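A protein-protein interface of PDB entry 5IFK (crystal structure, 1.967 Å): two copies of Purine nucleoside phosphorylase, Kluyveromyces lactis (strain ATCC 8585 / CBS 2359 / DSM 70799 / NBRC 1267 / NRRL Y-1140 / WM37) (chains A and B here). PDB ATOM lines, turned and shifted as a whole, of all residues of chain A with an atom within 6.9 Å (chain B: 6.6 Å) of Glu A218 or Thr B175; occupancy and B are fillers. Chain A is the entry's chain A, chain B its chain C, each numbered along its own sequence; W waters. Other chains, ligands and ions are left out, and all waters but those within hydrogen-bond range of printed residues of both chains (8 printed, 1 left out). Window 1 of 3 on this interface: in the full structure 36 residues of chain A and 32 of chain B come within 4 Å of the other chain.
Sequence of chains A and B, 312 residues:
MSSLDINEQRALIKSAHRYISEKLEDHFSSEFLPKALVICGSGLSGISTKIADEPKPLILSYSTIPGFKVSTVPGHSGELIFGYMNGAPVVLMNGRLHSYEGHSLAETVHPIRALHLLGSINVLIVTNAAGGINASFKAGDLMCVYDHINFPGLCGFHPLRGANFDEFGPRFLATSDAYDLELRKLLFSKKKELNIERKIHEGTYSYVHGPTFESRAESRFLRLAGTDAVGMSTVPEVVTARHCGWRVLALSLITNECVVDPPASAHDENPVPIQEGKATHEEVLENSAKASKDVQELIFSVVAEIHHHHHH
Of the 19 printed residues of chain B, 13 touch a printed residue of chain A.
Hydrophobic or aromatic side chains of chain B that line the printed part of chain A: His B148, Ile B149, His B158, Ala B174, Ala B225 and Val B239.
Among the printed residues, 26 pairs touch across the chains.
A ring nitrogen (NE2) of His B158 sits at hydrogen-bond distance from the side-chain hydroxyl (OG1) of Thr A212 (2.9 Å).
The backbone carbonyl oxygen of Ser B176 lies within hydrogen-bond range of the guanidinium group of Arg A216, 2.7 Å away.
The backbone NH of Phe A213 sits at hydrogen-bond distance from the backbone carbonyl oxygen of Leu B173, at 2.8 Å.
The side-chain carboxylate of Asp B147 is in hydrogen-bond range of the backbone NH of Ala A217 (2.8 Å).
The side-chain amino group (NZ) of Lys A278 is in salt-bridge range of the side-chain carboxylate (OD2) of Asp B177 (2.9 Å).
N of Ser A215 lies within hydrogen-bond range of OG1 of Thr B175, at 3.0 Å.
The side-chain carboxylate (OE2) of Glu A218 is in hydrogen-bond range of the backbone NH (N) of Asn B150.
The backbone carbonyl oxygen of His B148 sits at hydrogen-bond distance from the side-chain hydroxyl of Ser A215, at 2.6 Å.
The side-chain hydroxyl of Thr B175 is in hydrogen-bond range of the backbone carbonyl oxygen of Phe A213 (2.7 Å).
Glu A218 touches just these residues of chain B: His B148, Ile B149, Asn B150 and Thr B175.
Of chain A, only Thr A212, Phe A213, Glu A214, Ser A215 and Glu A218 come within 4 Å of Thr B175.
Of the printed residues of chain A, His B158 touches Thr A212 (2.9 Å).
Of the printed residues of chain A, Asp B177 touches Lys A278.
Leu A224 touches none of the printed residues of chain B.
The nearest printed residue of chain B that does not touch Ser A215 is Ser B176 (4.1 Å).
The backbone carbonyl oxygen of Ser A215 sits at hydrogen-bond distance from the side-chain hydroxyl of Ser A219 (3.2 Å).
OD2 of Asp B177 lies within salt-bridge range of NH2 of Arg B242, at 3.5 Å.
No position is printed for both chains.
Of the 26 pairs that touch across the chains among the printed residues, none has its exchanged pair printed and touching as well.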
ATOM      1  N   ILE A 133     -36.241   7.006  18.387  1.00  0.00           N
ATOM      2  CA  ILE A 133     -36.074   7.208  19.824  1.00  0.00           C
ATOM      3  C   ILE A 133     -37.208   8.070  20.355  1.00  0.00           C
ATOM      4  O   ILE A 133     -37.751   7.808  21.427  1.00  0.00           O
ATOM      5  CB  ILE A 133     -34.698   7.843  20.147  1.00  0.00           C
ATOM      6  CG1 ILE A 133     -33.570   6.855  19.842  1.00  0.00           C
ATOM      7  CG2 ILE A 133     -34.613   8.231  21.604  1.00  0.00           C
ATOM      8  CD1 ILE A 133     -33.466   5.707  20.863  1.00  0.00           C
ATOM      9  N   THR A 212     -23.815  -3.073  17.882  1.00  0.00           N
ATOM     10  CA  THR A 212     -24.966  -3.511  18.680  1.00  0.00           C
ATOM     11  C   THR A 212     -26.117  -2.544  18.493  1.00  0.00           C
ATOM     12  O   THR A 212     -25.894  -1.360  18.298  1.00  0.00           O
ATOM     13  CB  THR A 212     -24.651  -3.595  20.182  1.00  0.00           C
ATOM     14  OG1 THR A 212     -23.954  -2.406  20.597  1.00  0.00           O
ATOM     15  CG2 THR A 212     -23.813  -4.852  20.499  1.00  0.00           C
ATOM     16  N   PHE A 213     -27.344  -3.054  18.543  1.00  0.00           N
ATOM     17  CA  PHE A 213     -28.522  -2.212  18.749  1.00  0.00           C
ATOM     18  C   PHE A 213     -28.583  -1.831  20.226  1.00  0.00           C
ATOM     19  O   PHE A 213     -28.117  -2.587  21.083  1.00  0.00           O
ATOM     20  CB  PHE A 213     -29.814  -2.940  18.352  1.00  0.00           C
ATOM     21  CG  PHE A 213     -29.909  -3.281  16.895  1.00  0.00           C
ATOM     22  CD1 PHE A 213     -29.943  -2.284  15.933  1.00  0.00           C
ATOM     23  CD2 PHE A 213     -30.018  -4.610  16.487  1.00  0.00           C
ATOM     24  CE1 PHE A 213     -30.063  -2.609  14.576  1.00  0.00           C
ATOM     25  CE2 PHE A 213     -30.138  -4.937  15.149  1.00  0.00           C
ATOM     26  CZ  PHE A 213     -30.162  -3.937  14.191  1.00  0.00           C
ATOM     27  N   GLU A 214     -29.179  -0.681  20.527  1.00  0.00           N
ATOM     28  CA  GLU A 214     -29.152  -0.126  21.876  1.00  0.00           C
ATOM     29  C   GLU A 214     -29.919  -0.974  22.873  1.00  0.00           C
ATOM     30  O   GLU A 214     -30.999  -1.493  22.565  1.00  0.00           O
ATOM     31  CB  GLU A 214     -29.731   1.297  21.887  1.00  0.00           C
ATOM     32  CG  GLU A 214     -28.938   2.297  21.070  1.00  0.00           C
ATOM     33  CD  GLU A 214     -29.069   2.059  19.570  1.00  0.00           C
ATOM     34  OE1 GLU A 214     -28.097   2.351  18.845  1.00  0.00           O
ATOM     35  OE2 GLU A 214     -30.131   1.563  19.117  1.00  0.00           O
ATOM     36  N   SER A 215     -29.369  -1.106  24.076  1.00  0.00           N
ATOM     37  CA  SER A 215     -30.127  -1.692  25.183  1.00  0.00           C
ATOM     38  C   SER A 215     -31.305  -0.762  25.510  1.00  0.00           C
ATOM     39  O   SER A 215     -31.393   0.347  24.970  1.00  0.00           O
ATOM     40  CB  SER A 215     -29.237  -1.904  26.411  1.00  0.00           C
ATOM     41  OG  SER A 215     -28.779  -0.665  26.928  1.00  0.00           O
ATOM     42  N   ARG A 216     -32.218  -1.202  26.371  1.00  0.00           N
ATOM     43  CA  ARG A 216     -33.320  -0.326  26.771  1.00  0.00           C
ATOM     44  C   ARG A 216     -32.815   0.916  27.520  1.00  0.00           C
ATOM     45  O   ARG A 216     -33.234   2.038  27.250  1.00  0.00           O
ATOM     46  CB  ARG A 216     -34.305  -1.097  27.630  1.00  0.00           C
ATOM     47  CG  ARG A 216     -34.845  -2.326  26.949  1.00  0.00           C
ATOM     48  CD  ARG A 216     -35.085  -3.401  27.994  1.00  0.00           C
ATOM     49  NE  ARG A 216     -35.620  -4.614  27.400  1.00  0.00           N
ATOM     50  CZ  ARG A 216     -36.910  -4.820  27.171  1.00  0.00           C
ATOM     51  NH1 ARG A 216     -37.802  -3.891  27.493  1.00  0.00           N
ATOM     52  NH2 ARG A 216     -37.302  -5.960  26.618  1.00  0.00           N
ATOM     53  N   ALA A 217     -31.892   0.715  28.450  1.00  0.00           N
ATOM     54  CA  ALA A 217     -31.331   1.828  29.195  1.00  0.00           C
ATOM     55  C   ALA A 217     -30.556   2.770  28.274  1.00  0.00           C
ATOM     56  O   ALA A 217     -30.546   3.975  28.495  1.00  0.00           O
ATOM     57  CB  ALA A 217     -30.428   1.320  30.313  1.00  0.00           C
ATOM     58  N   GLU A 218     -29.903   2.222  27.248  1.00  0.00           N
ATOM     59  CA  GLU A 218     -29.154   3.066  26.305  1.00  0.00           C
ATOM     60  C   GLU A 218     -30.100   3.968  25.512  1.00  0.00           C
ATOM     61  O   GLU A 218     -29.813   5.163  25.320  1.00  0.00           O
ATOM     62  CB  GLU A 218     -28.308   2.206  25.349  1.00  0.00           C
ATOM     63  CG  GLU A 218     -27.001   1.721  25.986  1.00  0.00           C
ATOM     64  CD  GLU A 218     -26.376   0.512  25.302  1.00  0.00           C
ATOM     65  OE1 GLU A 218     -26.872   0.090  24.237  1.00  0.00           O
ATOM     66  OE2 GLU A 218     -25.376  -0.017  25.832  1.00  0.00           O
ATOM     67  N   SER A 219     -31.215   3.404  25.049  1.00  0.00           N
ATOM     68  CA  SER A 219     -32.206   4.186  24.293  1.00  0.00           C
ATOM     69  C   SER A 219     -32.847   5.262  25.160  1.00  0.00           C
ATOM     70  O   SER A 219     -33.081   6.395  24.712  1.00  0.00           O
ATOM     71  CB  SER A 219     -33.299   3.284  23.730  1.00  0.00           C
ATOM     72  OG  SER A 219     -32.761   2.351  22.826  1.00  0.00           O
ATOM     73  N   ARG A 220     -33.142   4.889  26.399  1.00  0.00           N
ATOM     74  CA  ARG A 220     -33.690   5.820  27.362  1.00  0.00           C
ATOM     75  C   ARG A 220     -32.709   6.968  27.593  1.00  0.00           C
ATOM     76  O   ARG A 220     -33.110   8.130  27.700  1.00  0.00           O
ATOM     77  CB  ARG A 220     -33.998   5.100  28.675  1.00  0.00           C
ATOM     78  CG  ARG A 220     -35.267   5.548  29.343  1.00  0.00           C
ATOM     79  CD  ARG A 220     -35.911   4.417  30.141  1.00  0.00           C
ATOM     80  NE  ARG A 220     -34.975   3.847  31.101  1.00  0.00           N
ATOM     81  CZ  ARG A 220     -34.635   2.562  31.157  1.00  0.00           C
ATOM     82  NH1 ARG A 220     -35.178   1.680  30.321  1.00  0.00           N
ATOM     83  NH2 ARG A 220     -33.758   2.158  32.070  1.00  0.00           N
ATOM     84  N   PHE A 221     -31.429   6.630  27.686  1.00  0.00           N
ATOM     85  CA  PHE A 221     -30.391   7.646  27.818  1.00  0.00           C
ATOM     86  C   PHE A 221     -30.390   8.577  26.608  1.00  0.00           C
ATOM     87  O   PHE A 221     -30.408   9.795  26.758  1.00  0.00           O
ATOM     88  CB  PHE A 221     -29.020   6.998  27.974  1.00  0.00           C
ATOM     89  CG  PHE A 221     -27.878   7.924  27.660  1.00  0.00           C
ATOM     90  CD1 PHE A 221     -27.663   9.056  28.426  1.00  0.00           C
ATOM     91  CD2 PHE A 221     -27.020   7.667  26.603  1.00  0.00           C
ATOM     92  CE1 PHE A 221     -26.610   9.911  28.153  1.00  0.00           C
ATOM     93  CE2 PHE A 221     -25.966   8.530  26.322  1.00  0.00           C
ATOM     94  CZ  PHE A 221     -25.765   9.647  27.103  1.00  0.00           C
ATOM     95  N   LEU A 222     -30.375   7.991  25.414  1.00  0.00           N
ATOM     96  CA  LEU A 222     -30.424   8.753  24.166  1.00  0.00           C
ATOM     97  C   LEU A 222     -31.656   9.666  24.129  1.00  0.00           C
ATOM     98  O   LEU A 222     -31.555  10.847  23.777  1.00  0.00           O
ATOM     99  CB  LEU A 222     -30.410   7.802  22.947  1.00  0.00           C
ATOM    100  CG  LEU A 222     -29.067   7.082  22.703  1.00  0.00           C
ATOM    101  CD1 LEU A 222     -29.145   6.072  21.543  1.00  0.00           C
ATOM    102  CD2 LEU A 222     -27.957   8.084  22.435  1.00  0.00           C
ATOM    103  N   ARG A 223     -32.809   9.136  24.520  1.00  0.00           N
ATOM    104  CA  ARG A 223     -34.039   9.936  24.525  1.00  0.00           C
ATOM    105  C   ARG A 223     -33.880  11.130  25.463  1.00  0.00           C
ATOM    106  O   ARG A 223     -34.134  12.268  25.099  1.00  0.00           O
ATOM    107  CB  ARG A 223     -35.243   9.085  24.940  1.00  0.00           C
ATOM    108  CG  ARG A 223     -36.588   9.839  24.924  1.00  0.00           C
ATOM    109  CD  ARG A 223     -37.739   8.924  25.302  1.00  0.00           C
ATOM    110  NE  ARG A 223     -38.129   8.033  24.214  1.00  0.00           N
ATOM    111  CZ  ARG A 223     -39.069   7.093  24.323  1.00  0.00           C
ATOM    112  NH1 ARG A 223     -39.699   6.911  25.476  1.00  0.00           N
ATOM    113  NH2 ARG A 223     -39.371   6.330  23.283  1.00  0.00           N
ATOM    114  N   LEU A 224     -33.420  10.837  26.668  1.00  0.00           N
ATOM    115  CA  LEU A 224     -33.155  11.838  27.686  1.00  0.00           C
ATOM    116  C   LEU A 224     -32.151  12.912  27.238  1.00  0.00           C
ATOM    117  O   LEU A 224     -32.267  14.089  27.594  1.00  0.00           O
ATOM    118  CB  LEU A 224     -32.640  11.112  28.908  1.00  0.00           C
ATOM    119  CG  LEU A 224     -32.456  11.828  30.215  1.00  0.00           C
ATOM    120  CD1 LEU A 224     -32.855  10.763  31.214  1.00  0.00           C
ATOM    121  CD2 LEU A 224     -30.998  12.222  30.379  1.00  0.00           C
ATOM    122  N   VAL A 259     -36.698  -0.110  21.654  1.00  0.00           N
ATOM    123  CA  VAL A 259     -37.272  -0.556  22.911  1.00  0.00           C
ATOM    124  C   VAL A 259     -36.673   0.280  24.039  1.00  0.00           C
ATOM    125  O   VAL A 259     -35.458   0.262  24.216  1.00  0.00           O
ATOM    126  CB  VAL A 259     -36.984  -2.051  23.162  1.00  0.00           C
ATOM    127  CG1 VAL A 259     -37.619  -2.510  24.470  1.00  0.00           C
ATOM    128  CG2 VAL A 259     -37.469  -2.889  21.982  1.00  0.00           C
ATOM    129  N   VAL A 260     -37.513   1.014  24.775  1.00  0.00           N
ATOM    130  CA  VAL A 260     -37.048   1.857  25.882  1.00  0.00           C
ATOM    131  C   VAL A 260     -37.585   1.437  27.253  1.00  0.00           C
ATOM    132  O   VAL A 260     -36.987   1.771  28.272  1.00  0.00           O
ATOM    133  CB  VAL A 260     -37.432   3.329  25.676  1.00  0.00           C
ATOM    134  CG1 VAL A 260     -36.659   3.927  24.515  1.00  0.00           C
ATOM    135  CG2 VAL A 260     -38.937   3.462  25.455  1.00  0.00           C
ATOM    136  N   LYS A 278     -37.516  -6.965  19.848  1.00  0.00           N
ATOM    137  CA  LYS A 278     -36.077  -6.700  19.724  1.00  0.00           C
ATOM    138  C   LYS A 278     -35.712  -6.330  18.282  1.00  0.00           C
ATOM    139  O   LYS A 278     -36.223  -6.923  17.332  1.00  0.00           O
ATOM    140  CB  LYS A 278     -35.243  -7.899  20.195  1.00  0.00           C
ATOM    141  CG  LYS A 278     -35.403  -9.144  19.350  1.00  0.00           C
ATOM    142  CD  LYS A 278     -34.707 -10.343  19.967  1.00  0.00           C
ATOM    143  CE  LYS A 278     -33.204 -10.283  19.779  1.00  0.00           C
ATOM    144  NZ  LYS A 278     -32.578 -11.568  20.208  1.00  0.00           N
ATOM    145  N   ALA A 279     -34.852  -5.330  18.132  1.00  0.00           N
ATOM    146  CA  ALA A 279     -34.392  -4.906  16.811  1.00  0.00           C
ATOM    147  C   ALA A 279     -33.660  -6.047  16.115  1.00  0.00           C
ATOM    148  O   ALA A 279     -32.929  -6.814  16.757  1.00  0.00           O
ATOM    149  CB  ALA A 279     -33.491  -3.682  16.913  1.00  0.00           C
ATOM    150  N   ASP B 147     -30.116  -4.740  33.027  1.00  0.00           N
ATOM    151  CA  ASP B 147     -29.880  -3.875  31.866  1.00  0.00           C
ATOM    152  C   ASP B 147     -28.542  -3.162  32.020  1.00  0.00           C
ATOM    153  O   ASP B 147     -28.011  -3.060  33.127  1.00  0.00           O
ATOM    154  CB  ASP B 147     -31.001  -2.851  31.730  1.00  0.00           C
ATOM    155  CG  ASP B 147     -31.160  -2.330  30.311  1.00  0.00           C
ATOM    156  OD1 ASP B 147     -30.423  -2.777  29.409  1.00  0.00           O
ATOM    157  OD2 ASP B 147     -32.052  -1.490  30.089  1.00  0.00           O
ATOM    158  N   HIS B 148     -27.986  -2.667  30.922  1.00  0.00           N
ATOM    159  CA  HIS B 148     -26.744  -1.904  31.042  1.00  0.00           C
ATOM    160  C   HIS B 148     -26.653  -0.746  30.074  1.00  0.00           C
ATOM    161  O   HIS B 148     -27.395  -0.673  29.090  1.00  0.00           O
ATOM    162  CB  HIS B 148     -25.511  -2.814  30.894  1.00  0.00           C
ATOM    163  CG  HIS B 148     -25.354  -3.464  29.550  1.00  0.00           C
ATOM    164  ND1 HIS B 148     -25.388  -2.762  28.362  1.00  0.00           N
ATOM    165  CD2 HIS B 148     -25.084  -4.747  29.215  1.00  0.00           C
ATOM    166  CE1 HIS B 148     -25.216  -3.596  27.352  1.00  0.00           C
ATOM    167  NE2 HIS B 148     -25.025  -4.805  27.844  1.00  0.00           N
ATOM    168  N   ILE B 149     -25.749   0.178  30.376  1.00  0.00           N
ATOM    169  CA  ILE B 149     -25.348   1.163  29.385  1.00  0.00           C
ATOM    170  C   ILE B 149     -23.870   0.926  29.084  1.00  0.00           C
ATOM    171  O   ILE B 149     -23.028   0.969  29.979  1.00  0.00           O
ATOM    172  CB  ILE B 149     -25.572   2.614  29.869  1.00  0.00           C
ATOM    173  CG1 ILE B 149     -27.055   2.861  30.170  1.00  0.00           C
ATOM    174  CG2 ILE B 149     -25.049   3.634  28.810  1.00  0.00           C
ATOM    175  CD1 ILE B 149     -27.308   4.126  30.968  1.00  0.00           C
ATOM    176  N   ASN B 150     -23.558   0.668  27.822  1.00  0.00           N
ATOM    177  CA  ASN B 150     -22.180   0.451  27.420  1.00  0.00           C
ATOM    178  C   ASN B 150     -21.562   1.765  26.916  1.00  0.00           C
ATOM    179  O   ASN B 150     -21.537   2.014  25.711  1.00  0.00           O
ATOM    180  CB  ASN B 150     -22.129  -0.637  26.348  1.00  0.00           C
ATOM    181  CG  ASN B 150     -20.712  -1.010  25.946  1.00  0.00           C
ATOM    182  OD1 ASN B 150     -19.732  -0.475  26.468  1.00  0.00           O
ATOM    183  ND2 ASN B 150     -20.602  -1.944  25.009  1.00  0.00           N
ATOM    184  N   PHE B 151     -21.096   2.614  27.830  1.00  0.00           N
ATOM    185  CA  PHE B 151     -20.629   3.935  27.415  1.00  0.00           C
ATOM    186  C   PHE B 151     -19.451   3.872  26.442  1.00  0.00           C
ATOM    187  O   PHE B 151     -19.509   4.512  25.386  1.00  0.00           O
ATOM    188  CB  PHE B 151     -20.293   4.805  28.638  1.00  0.00           C
ATOM    189  CG  PHE B 151     -21.511   5.422  29.265  1.00  0.00           C
ATOM    190  CD1 PHE B 151     -22.160   6.480  28.636  1.00  0.00           C
ATOM    191  CD2 PHE B 151     -22.032   4.931  30.455  1.00  0.00           C
ATOM    192  CE1 PHE B 151     -23.293   7.060  29.207  1.00  0.00           C
ATOM    193  CE2 PHE B 151     -23.172   5.503  31.025  1.00  0.00           C
ATOM    194  CZ  PHE B 151     -23.794   6.573  30.401  1.00  0.00           C
ATOM    195  N   LEU B 154     -20.689   2.865  22.931  1.00  0.00           N
ATOM    196  CA  LEU B 154     -21.357   3.869  22.112  1.00  0.00           C
ATOM    197  C   LEU B 154     -20.350   4.706  21.329  1.00  0.00           C
ATOM    198  O   LEU B 154     -20.671   5.231  20.251  1.00  0.00           O
ATOM    199  CB  LEU B 154     -22.239   4.778  22.986  1.00  0.00           C
ATOM    200  CG  LEU B 154     -23.433   4.097  23.670  1.00  0.00           C
ATOM    201  CD1 LEU B 154     -24.159   5.053  24.611  1.00  0.00           C
ATOM    202  CD2 LEU B 154     -24.405   3.512  22.632  1.00  0.00           C
ATOM    203  N   HIS B 158     -15.577  -1.007  21.546  1.00  0.00           N
ATOM    204  CA  HIS B 158     -16.629  -2.020  21.483  1.00  0.00           C
ATOM    205  C   HIS B 158     -16.015  -3.384  21.161  1.00  0.00           C
ATOM    206  O   HIS B 158     -15.202  -3.485  20.242  1.00  0.00           O
ATOM    207  CB  HIS B 158     -17.647  -1.607  20.418  1.00  0.00           C
ATOM    208  CG  HIS B 158     -18.971  -2.294  20.521  1.00  0.00           C
ATOM    209  ND1 HIS B 158     -19.129  -3.645  20.298  1.00  0.00           N
ATOM    210  CD2 HIS B 158     -20.210  -1.807  20.775  1.00  0.00           C
ATOM    211  CE1 HIS B 158     -20.403  -3.968  20.441  1.00  0.00           C
ATOM    212  NE2 HIS B 158     -21.081  -2.870  20.728  1.00  0.00           N
ATOM    213  N   LEU B 173     -26.054  -7.034  16.709  1.00  0.00           N
ATOM    214  CA  LEU B 173     -26.537  -7.777  17.863  1.00  0.00           C
ATOM    215  C   LEU B 173     -27.481  -6.923  18.699  1.00  0.00           C
ATOM    216  O   LEU B 173     -27.118  -5.826  19.124  1.00  0.00           O
ATOM    217  CB  LEU B 173     -25.357  -8.260  18.721  1.00  0.00           C
ATOM    218  CG  LEU B 173     -25.742  -8.940  20.040  1.00  0.00           C
ATOM    219  CD1 LEU B 173     -26.489 -10.250  19.786  1.00  0.00           C
ATOM    220  CD2 LEU B 173     -24.519  -9.163  20.921  1.00  0.00           C
ATOM    221  N   ALA B 174     -28.693  -7.415  18.936  1.00  0.00           N
ATOM    222  CA  ALA B 174     -29.587  -6.711  19.840  1.00  0.00           C
ATOM    223  C   ALA B 174     -29.100  -6.878  21.271  1.00  0.00           C
ATOM    224  O   ALA B 174     -28.625  -7.951  21.640  1.00  0.00           O
ATOM    225  CB  ALA B 174     -31.014  -7.220  19.690  1.00  0.00           C
ATOM    226  N   THR B 175     -29.212  -5.827  22.082  1.00  0.00           N
ATOM    227  CA  THR B 175     -28.846  -5.942  23.492  1.00  0.00           C
ATOM    228  C   THR B 175     -29.997  -5.596  24.451  1.00  0.00           C
ATOM    229  O   THR B 175     -29.796  -5.564  25.666  1.00  0.00           O
ATOM    230  CB  THR B 175     -27.629  -5.051  23.852  1.00  0.00           C
ATOM    231  OG1 THR B 175     -27.906  -3.683  23.526  1.00  0.00           O
ATOM    232  CG2 THR B 175     -26.360  -5.527  23.123  1.00  0.00           C
ATOM    233  N   SER B 176     -31.199  -5.393  23.928  1.00  0.00           N
ATOM    234  CA  SER B 176     -32.348  -5.145  24.799  1.00  0.00           C
ATOM    235  C   SER B 176     -32.812  -6.395  25.575  1.00  0.00           C
ATOM    236  O   SER B 176     -33.671  -6.295  26.456  1.00  0.00           O
ATOM    237  CB  SER B 176     -33.517  -4.578  23.998  1.00  0.00           C
ATOM    238  OG  SER B 176     -33.943  -5.470  22.985  1.00  0.00           O
ATOM    239  N   ASP B 177     -32.234  -7.554  25.260  1.00  0.00           N
ATOM    240  CA  ASP B 177     -32.595  -8.808  25.925  1.00  0.00           C
ATOM    241  C   ASP B 177     -31.368  -9.498  26.506  1.00  0.00           C
ATOM    242  O   ASP B 177     -31.273 -10.724  26.490  1.00  0.00           O
ATOM    243  CB  ASP B 177     -33.299  -9.749  24.941  1.00  0.00           C
ATOM    244  CG  ASP B 177     -32.451 -10.043  23.712  1.00  0.00           C
ATOM    245  OD1 ASP B 177     -31.516  -9.265  23.435  1.00  0.00           O
ATOM    246  OD2 ASP B 177     -32.716 -11.036  23.010  1.00  0.00           O
ATOM    247  N   ALA B 178     -30.430  -8.709  27.016  1.00  0.00           N
ATOM    248  CA  ALA B 178     -29.135  -9.243  27.408  1.00  0.00           C
ATOM    249  C   ALA B 178     -29.177 -10.085  28.693  1.00  0.00           C
ATOM    250  O   ALA B 178     -28.426 -11.052  28.814  1.00  0.00           O
ATOM    251  CB  ALA B 178     -28.133  -8.109  27.557  1.00  0.00           C
ATOM    252  N   TYR B 179     -30.046  -9.737  29.638  1.00  0.00           N
ATOM    253  CA  TYR B 179     -29.977 -10.359  30.964  1.00  0.00           C
ATOM    254  C   TYR B 179     -31.185 -11.246  31.219  1.00  0.00           C
ATOM    255  O   TYR B 179     -32.237 -10.773  31.653  1.00  0.00           O
ATOM    256  CB  TYR B 179     -29.837  -9.288  32.054  1.00  0.00           C
ATOM    257  CG  TYR B 179     -28.563  -8.489  31.898  1.00  0.00           C
ATOM    258  CD1 TYR B 179     -27.358  -8.955  32.429  1.00  0.00           C
ATOM    259  CD2 TYR B 179     -28.549  -7.305  31.171  1.00  0.00           C
ATOM    260  CE1 TYR B 179     -26.184  -8.252  32.268  1.00  0.00           C
ATOM    261  CE2 TYR B 179     -27.369  -6.586  31.003  1.00  0.00           C
ATOM    262  CZ  TYR B 179     -26.191  -7.075  31.560  1.00  0.00           C
ATOM    263  OH  TYR B 179     -25.007  -6.394  31.422  1.00  0.00           O
ATOM    264  N   THR B 204     -29.971  -1.080  36.563  1.00  0.00           N
ATOM    265  CA  THR B 204     -29.139  -0.827  35.396  1.00  0.00           C
ATOM    266  C   THR B 204     -27.690  -0.597  35.784  1.00  0.00           C
ATOM    267  O   THR B 204     -27.386   0.253  36.633  1.00  0.00           O
ATOM    268  CB  THR B 204     -29.639   0.385  34.629  1.00  0.00           C
ATOM    269  OG1 THR B 204     -30.961   0.125  34.191  1.00  0.00           O
ATOM    270  CG2 THR B 204     -28.752   0.678  33.407  1.00  0.00           C
ATOM    271  N   ALA B 225     -28.692   9.722  33.725  1.00  0.00           N
ATOM    272  CA  ALA B 225     -28.709   8.865  32.543  1.00  0.00           C
ATOM    273  C   ALA B 225     -29.477   7.558  32.771  1.00  0.00           C
ATOM    274  O   ALA B 225     -29.760   6.847  31.813  1.00  0.00           O
ATOM    275  CB  ALA B 225     -27.293   8.571  32.102  1.00  0.00           C
ATOM    276  N   VAL B 235     -19.402  -5.585  31.104  1.00  0.00           N
ATOM    277  CA  VAL B 235     -20.274  -5.402  29.943  1.00  0.00           C
ATOM    278  C   VAL B 235     -19.668  -5.930  28.621  1.00  0.00           C
ATOM    279  O   VAL B 235     -20.384  -6.575  27.857  1.00  0.00           O
ATOM    280  CB  VAL B 235     -20.702  -3.918  29.815  1.00  0.00           C
ATOM    281  CG1 VAL B 235     -21.222  -3.593  28.397  1.00  0.00           C
ATOM    282  CG2 VAL B 235     -21.792  -3.605  30.861  1.00  0.00           C
ATOM    283  N   VAL B 239     -21.553  -8.664  26.411  1.00  0.00           N
ATOM    284  CA  VAL B 239     -21.904  -8.460  25.008  1.00  0.00           C
ATOM    285  C   VAL B 239     -21.348  -9.581  24.134  1.00  0.00           C
ATOM    286  O   VAL B 239     -22.007 -10.057  23.192  1.00  0.00           O
ATOM    287  CB  VAL B 239     -21.396  -7.094  24.487  1.00  0.00           C
ATOM    288  CG1 VAL B 239     -21.549  -7.032  22.956  1.00  0.00           C
ATOM    289  CG2 VAL B 239     -22.198  -5.966  25.124  1.00  0.00           C
ATOM    290  N   ARG B 242     -23.332 -12.770  24.766  1.00  0.00           N
ATOM    291  CA  ARG B 242     -24.608 -12.649  24.060  1.00  0.00           C
ATOM    292  C   ARG B 242     -24.423 -12.863  22.560  1.00  0.00           C
ATOM    293  O   ARG B 242     -25.251 -13.499  21.914  1.00  0.00           O
ATOM    294  CB  ARG B 242     -25.243 -11.295  24.342  1.00  0.00           C
ATOM    295  CG  ARG B 242     -25.833 -11.200  25.734  1.00  0.00           C
ATOM    296  CD  ARG B 242     -26.876 -12.283  25.912  1.00  0.00           C
ATOM    297  NE  ARG B 242     -27.941 -12.111  24.938  1.00  0.00           N
ATOM    298  CZ  ARG B 242     -28.757 -13.070  24.526  1.00  0.00           C
ATOM    299  NH1 ARG B 242     -28.622 -14.308  24.988  1.00  0.00           N
ATOM    300  NH2 ARG B 242     -29.708 -12.785  23.639  1.00  0.00           N
HETATM  301  O   HOH W   1     -29.883 -10.901  21.282  1.00  0.00           O
HETATM  302  O   HOH W   2     -33.554  -4.364  20.466  1.00  0.00           O
HETATM  303  O   HOH W   3     -22.717   0.058  22.460  1.00  0.00           O
HETATM  304  O   HOH W   4     -31.236  -3.879  21.285  1.00  0.00           O
HETATM  305  O   HOH W   5     -23.044  -2.563  23.456  1.00  0.00           O
HETATM  306  O   HOH W   6     -33.811  -0.348  31.844  1.00  0.00           O
HETATM  307  O   HOH W   7     -31.138   4.924  30.968  1.00  0.00           O
HETATM  308  O   HOH W   8     -25.259  -2.553  24.714  1.00  0.00           O
